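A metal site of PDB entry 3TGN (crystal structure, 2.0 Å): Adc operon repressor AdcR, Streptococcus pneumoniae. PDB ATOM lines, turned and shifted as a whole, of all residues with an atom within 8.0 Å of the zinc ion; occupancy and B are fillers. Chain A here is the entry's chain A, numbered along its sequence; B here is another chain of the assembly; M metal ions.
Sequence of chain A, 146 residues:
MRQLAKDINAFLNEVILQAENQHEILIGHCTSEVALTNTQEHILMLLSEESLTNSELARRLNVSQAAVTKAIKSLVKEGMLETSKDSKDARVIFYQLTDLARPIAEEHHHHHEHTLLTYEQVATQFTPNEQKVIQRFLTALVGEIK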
ATOM      1  N   GLN A  22      26.378 -14.957   8.724  1.00  0.00           N
ATOM      2  CA  GLN A  22      25.486 -16.111   8.842  1.00  0.00           C
ATOM      3  C   GLN A  22      25.943 -17.278   7.970  1.00  0.00           C
ATOM      4  O   GLN A  22      26.793 -17.118   7.092  1.00  0.00           O
ATOM      5  CB  GLN A  22      24.051 -15.719   8.464  1.00  0.00           C
ATOM      6  CG  GLN A  22      23.529 -14.483   9.175  1.00  0.00           C
ATOM      7  CD  GLN A  22      22.188 -14.028   8.626  1.00  0.00           C
ATOM      8  OE1 GLN A  22      21.600 -14.685   7.760  1.00  0.00           O
ATOM      9  NE2 GLN A  22      21.693 -12.900   9.117  1.00  0.00           N
ATOM     10  N   HIS A  23      25.375 -18.457   8.205  1.00  0.00           N
ATOM     11  CA  HIS A  23      25.709 -19.642   7.440  1.00  0.00           C
ATOM     12  C   HIS A  23      24.657 -19.935   6.369  1.00  0.00           C
ATOM     13  O   HIS A  23      24.751 -20.925   5.638  1.00  0.00           O
ATOM     14  CB  HIS A  23      25.851 -20.863   8.350  1.00  0.00           C
ATOM     15  CG  HIS A  23      24.551 -21.549   8.637  1.00  0.00           C
ATOM     16  ND1 HIS A  23      23.554 -20.978   9.400  1.00  0.00           N
ATOM     17  CD2 HIS A  23      24.085 -22.767   8.273  1.00  0.00           C
ATOM     18  CE1 HIS A  23      22.531 -21.805   9.494  1.00  0.00           C
ATOM     19  NE2 HIS A  23      22.833 -22.903   8.819  1.00  0.00           N
ATOM     20  N   GLU A  24      23.647 -19.086   6.295  1.00  0.00           N
ATOM     21  CA  GLU A  24      22.521 -19.319   5.402  1.00  0.00           C
ATOM     22  C   GLU A  24      21.834 -18.019   5.038  1.00  0.00           C
ATOM     23  O   GLU A  24      21.952 -17.015   5.745  1.00  0.00           O
ATOM     24  CB  GLU A  24      21.503 -20.236   6.077  1.00  0.00           C
ATOM     25  CG  GLU A  24      20.870 -19.596   7.307  1.00  0.00           C
ATOM     26  CD  GLU A  24      19.900 -20.509   8.036  1.00  0.00           C
ATOM     27  OE1 GLU A  24      19.337 -20.054   9.053  1.00  0.00           O
ATOM     28  OE2 GLU A  24      19.717 -21.671   7.602  1.00  0.00           O
ATOM     29  N   ILE A  25      21.107 -18.035   3.929  1.00  0.00           N
ATOM     30  CA  ILE A  25      20.276 -16.911   3.541  1.00  0.00           C
ATOM     31  C   ILE A  25      18.818 -17.254   3.791  1.00  0.00           C
ATOM     32  O   ILE A  25      18.363 -18.351   3.462  1.00  0.00           O
ATOM     33  CB  ILE A  25      20.455 -16.560   2.060  1.00  0.00           C
ATOM     34  CG1 ILE A  25      21.701 -15.684   1.872  1.00  0.00           C
ATOM     35  CG2 ILE A  25      19.214 -15.831   1.542  1.00  0.00           C
ATOM     36  CD1 ILE A  25      21.899 -15.222   0.455  1.00  0.00           C
ATOM     37  N   LEU A  26      18.083 -16.315   4.389  1.00  0.00           N
ATOM     38  CA  LEU A  26      16.643 -16.454   4.556  1.00  0.00           C
ATOM     39  C   LEU A  26      15.935 -15.309   3.859  1.00  0.00           C
ATOM     40  O   LEU A  26      16.485 -14.211   3.757  1.00  0.00           O
ATOM     41  CB  LEU A  26      16.287 -16.489   6.043  1.00  0.00           C
ATOM     42  CG  LEU A  26      16.826 -17.683   6.831  1.00  0.00           C
ATOM     43  CD1 LEU A  26      16.614 -17.490   8.325  1.00  0.00           C
ATOM     44  CD2 LEU A  26      16.189 -18.978   6.347  1.00  0.00           C
ATOM     45  N   ASN A  38      21.202 -14.919  13.680  1.00  0.00           N
ATOM     46  CA  ASN A  38      20.568 -15.967  12.904  1.00  0.00           C
ATOM     47  C   ASN A  38      21.083 -17.341  13.301  1.00  0.00           C
ATOM     48  O   ASN A  38      20.334 -18.313  13.358  1.00  0.00           O
ATOM     49  CB  ASN A  38      20.786 -15.748  11.402  1.00  0.00           C
ATOM     50  CG  ASN A  38      20.018 -16.745  10.567  1.00  0.00           C
ATOM     51  OD1 ASN A  38      18.822 -16.577  10.336  1.00  0.00           O
ATOM     52  ND2 ASN A  38      20.700 -17.801  10.122  1.00  0.00           N
ATOM     53  N   THR A  39      22.378 -17.417  13.593  1.00  0.00           N
ATOM     54  CA  THR A  39      22.972 -18.690  14.017  1.00  0.00           C
ATOM     55  C   THR A  39      22.345 -19.169  15.325  1.00  0.00           C
ATOM     56  O   THR A  39      22.035 -20.350  15.484  1.00  0.00           O
ATOM     57  CB  THR A  39      24.506 -18.573  14.153  1.00  0.00           C
ATOM     58  OG1 THR A  39      25.078 -18.297  12.869  1.00  0.00           O
ATOM     59  CG2 THR A  39      25.088 -19.862  14.696  1.00  0.00           C
ATOM     60  N   GLU A  41      19.287 -18.438  16.464  1.00  0.00           N
ATOM     61  CA  GLU A  41      17.945 -18.916  16.152  1.00  0.00           C
ATOM     62  C   GLU A  41      17.969 -20.302  15.508  1.00  0.00           C
ATOM     63  O   GLU A  41      17.171 -21.174  15.855  1.00  0.00           O
ATOM     64  CB  GLU A  41      17.192 -17.945  15.246  1.00  0.00           C
ATOM     65  CG  GLU A  41      16.797 -16.639  15.927  1.00  0.00           C
ATOM     66  CD  GLU A  41      15.643 -15.938  15.232  1.00  0.00           C
ATOM     67  OE1 GLU A  41      15.176 -16.446  14.188  1.00  0.00           O
ATOM     68  OE2 GLU A  41      15.204 -14.883  15.724  1.00  0.00           O
ATOM     69  N   HIS A  42      18.901 -20.500  14.581  1.00  0.00           N
ATOM     70  CA  HIS A  42      19.004 -21.774  13.887  1.00  0.00           C
ATOM     71  C   HIS A  42      19.360 -22.888  14.874  1.00  0.00           C
ATOM     72  O   HIS A  42      18.801 -23.984  14.823  1.00  0.00           O
ATOM     73  CB  HIS A  42      20.040 -21.706  12.756  1.00  0.00           C
ATOM     74  CG  HIS A  42      19.950 -22.861  11.805  1.00  0.00           C
ATOM     75  ND1 HIS A  42      19.176 -22.835  10.674  1.00  0.00           N
ATOM     76  CD2 HIS A  42      20.543 -24.083  11.834  1.00  0.00           C
ATOM     77  CE1 HIS A  42      19.289 -23.993  10.043  1.00  0.00           C
ATOM     78  NE2 HIS A  42      20.115 -24.766  10.722  1.00  0.00           N
ATOM     79  N   ILE A  43      20.291 -22.601  15.771  1.00  0.00           N
ATOM     80  CA  ILE A  43      20.648 -23.569  16.806  1.00  0.00           C
ATOM     81  C   ILE A  43      19.450 -23.901  17.695  1.00  0.00           C
ATOM     82  O   ILE A  43      19.236 -25.059  18.037  1.00  0.00           O
ATOM     83  CB  ILE A  43      21.850 -23.081  17.652  1.00  0.00           C
ATOM     84  CG1 ILE A  43      23.125 -23.129  16.810  1.00  0.00           C
ATOM     85  CG2 ILE A  43      22.001 -23.925  18.918  1.00  0.00           C
ATOM     86  CD1 ILE A  43      24.315 -22.466  17.457  1.00  0.00           C
ATOM     87  N   MET A  45      16.332 -23.784  16.745  1.00  0.00           N
ATOM     88  CA  MET A  45      15.452 -24.587  15.906  1.00  0.00           C
ATOM     89  C   MET A  45      15.874 -26.051  15.944  1.00  0.00           C
ATOM     90  O   MET A  45      15.040 -26.937  16.155  1.00  0.00           O
ATOM     91  CB  MET A  45      15.442 -24.072  14.462  1.00  0.00           C
ATOM     92  CG  MET A  45      14.463 -24.793  13.572  1.00  0.00           C
ATOM     93  SD  MET A  45      14.533 -24.284  11.848  1.00  0.00           S
ATOM     94  CE  MET A  45      16.135 -24.932  11.384  1.00  0.00           C
ATOM     95  N   LEU A  46      17.155 -26.293  15.741  1.00  0.00           N
ATOM     96  CA  LEU A  46      17.667 -27.668  15.702  1.00  0.00           C
ATOM     97  C   LEU A  46      17.513 -28.371  17.051  1.00  0.00           C
ATOM     98  O   LEU A  46      17.089 -29.523  17.110  1.00  0.00           O
ATOM     99  CB  LEU A  46      19.128 -27.691  15.251  1.00  0.00           C
ATOM    100  CG  LEU A  46      19.420 -27.212  13.820  1.00  0.00           C
ATOM    101  CD1 LEU A  46      20.868 -27.500  13.438  1.00  0.00           C
ATOM    102  CD2 LEU A  46      18.476 -27.866  12.823  1.00  0.00           C
ATOM    103  N   LEU A  61      25.486 -27.046  10.648  1.00  0.00           N
ATOM    104  CA  LEU A  61      25.511 -25.692  10.088  1.00  0.00           C
ATOM    105  C   LEU A  61      26.703 -25.472   9.181  1.00  0.00           C
ATOM    106  O   LEU A  61      26.756 -24.478   8.446  1.00  0.00           O
ATOM    107  CB  LEU A  61      25.543 -24.638  11.196  1.00  0.00           C
ATOM    108  CG  LEU A  61      24.246 -24.406  11.977  1.00  0.00           C
ATOM    109  CD1 LEU A  61      24.010 -25.527  12.981  1.00  0.00           C
ATOM    110  CD2 LEU A  61      24.296 -23.060  12.680  1.00  0.00           C
ATOM    111  N   HIS A 108      11.705 -19.300  13.544  1.00  0.00           N
ATOM    112  CA  HIS A 108      12.838 -19.567  12.653  1.00  0.00           C
ATOM    113  C   HIS A 108      12.501 -20.685  11.685  1.00  0.00           C
ATOM    114  O   HIS A 108      12.942 -20.676  10.530  1.00  0.00           O
ATOM    115  CB  HIS A 108      14.102 -19.904  13.443  1.00  0.00           C
ATOM    116  CG  HIS A 108      15.340 -19.936  12.604  1.00  0.00           C
ATOM    117  ND1 HIS A 108      15.998 -18.805  12.202  1.00  0.00           N
ATOM    118  CD2 HIS A 108      16.032 -20.985  12.081  1.00  0.00           C
ATOM    119  CE1 HIS A 108      17.056 -19.139  11.466  1.00  0.00           C
ATOM    120  NE2 HIS A 108      17.086 -20.458  11.375  1.00  0.00           N
ATOM    121  N   HIS A 109      11.721 -21.655  12.141  1.00  0.00           N
ATOM    122  CA  HIS A 109      11.245 -22.731  11.285  1.00  0.00           C
ATOM    123  C   HIS A 109      10.296 -22.188  10.214  1.00  0.00           C
ATOM    124  O   HIS A 109      10.342 -22.606   9.060  1.00  0.00           O
ATOM    125  CB  HIS A 109      10.530 -23.801  12.120  1.00  0.00           C
ATOM    126  CG  HIS A 109       9.935 -24.905  11.304  1.00  0.00           C
ATOM    127  ND1 HIS A 109      10.700 -25.907  10.744  1.00  0.00           N
ATOM    128  CD2 HIS A 109       8.655 -25.160  10.943  1.00  0.00           C
ATOM    129  CE1 HIS A 109       9.906 -26.736  10.084  1.00  0.00           C
ATOM    130  NE2 HIS A 109       8.668 -26.308  10.194  1.00  0.00           N
ATOM    131  N   HIS A 111      10.269 -19.178   9.103  1.00  0.00           N
ATOM    132  CA  HIS A 111      11.091 -18.360   8.222  1.00  0.00           C
ATOM    133  C   HIS A 111      11.703 -19.243   7.145  1.00  0.00           C
ATOM    134  O   HIS A 111      11.716 -18.886   5.972  1.00  0.00           O
ATOM    135  CB  HIS A 111      12.179 -17.651   9.027  1.00  0.00           C
ATOM    136  CG  HIS A 111      12.688 -16.402   8.391  1.00  0.00           C
ATOM    137  ND1 HIS A 111      13.602 -15.566   9.000  1.00  0.00           N
ATOM    138  CD2 HIS A 111      12.393 -15.821   7.197  1.00  0.00           C
ATOM    139  CE1 HIS A 111      13.860 -14.549   8.213  1.00  0.00           C
ATOM    140  NE2 HIS A 111      13.141 -14.675   7.115  1.00  0.00           N
ATOM    141  N   HIS A 112      12.184 -20.420   7.550  1.00  0.00           N
ATOM    142  CA  HIS A 112      12.710 -21.391   6.595  1.00  0.00           C
ATOM    143  C   HIS A 112      11.645 -21.847   5.595  1.00  0.00           C
ATOM    144  O   HIS A 112      11.915 -21.974   4.401  1.00  0.00           O
ATOM    145  CB  HIS A 112      13.304 -22.602   7.316  1.00  0.00           C
ATOM    146  CG  HIS A 112      14.746 -22.448   7.660  1.00  0.00           C
ATOM    147  ND1 HIS A 112      15.762 -22.867   6.831  1.00  0.00           N
ATOM    148  CD2 HIS A 112      15.351 -21.907   8.739  1.00  0.00           C
ATOM    149  CE1 HIS A 112      16.926 -22.600   7.385  1.00  0.00           C
ATOM    150  NE2 HIS A 112      16.711 -22.020   8.547  1.00  0.00           N
ATOM    151  N   ASN B  13      23.491 -22.309   0.503  1.00  0.00           N
ATOM    152  CA  ASN B  13      24.269 -22.851   1.625  1.00  0.00           C
ATOM    153  C   ASN B  13      25.717 -23.112   1.228  1.00  0.00           C
ATOM    154  O   ASN B  13      26.640 -22.747   1.954  1.00  0.00           O
ATOM    155  CB  ASN B  13      23.645 -24.146   2.143  1.00  0.00           C
ATOM    156  CG  ASN B  13      22.423 -23.904   3.003  1.00  0.00           C
ATOM    157  OD1 ASN B  13      21.985 -22.777   3.170  1.00  0.00           O
ATOM    158  ND2 ASN B  13      21.863 -24.980   3.545  1.00  0.00           N
HETATM  159 ZN    ZN M   1      18.083 -21.349   9.820  1.00  0.00          ZN
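A ring nitrogen (ND1) of His 108 sits close to the side-chain carboxylate (OE1) of Glu 41 (3.2 Å). The side-chain amide oxygen of Gln 22 lies close to the backbone carbonyl oxygen of Glu 24 (3.1 Å). The side-chain carboxylate (OE1) of Glu 24 sits close to the side-chain amide nitrogen (ND2) of Asn 38 (2.8 Å).
Within 4 Å of the zinc ion: Glu 24, His 42, His 108 and His 112.
The zinc ion is bound by the side-chain carboxylate of Glu 24 (2.0 Å), a ring nitrogen (NE2) of His 112 (2.0 Å), a ring nitrogen (ND1) of His 42 (2.0 Å) and a ring nitrogen (NE2) of His 108 (2.1 Å). The zinc ion has four donor atoms within binding distance. Slightly farther from the zinc ion lies OE2 of Glu 24 (2.8 Å).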
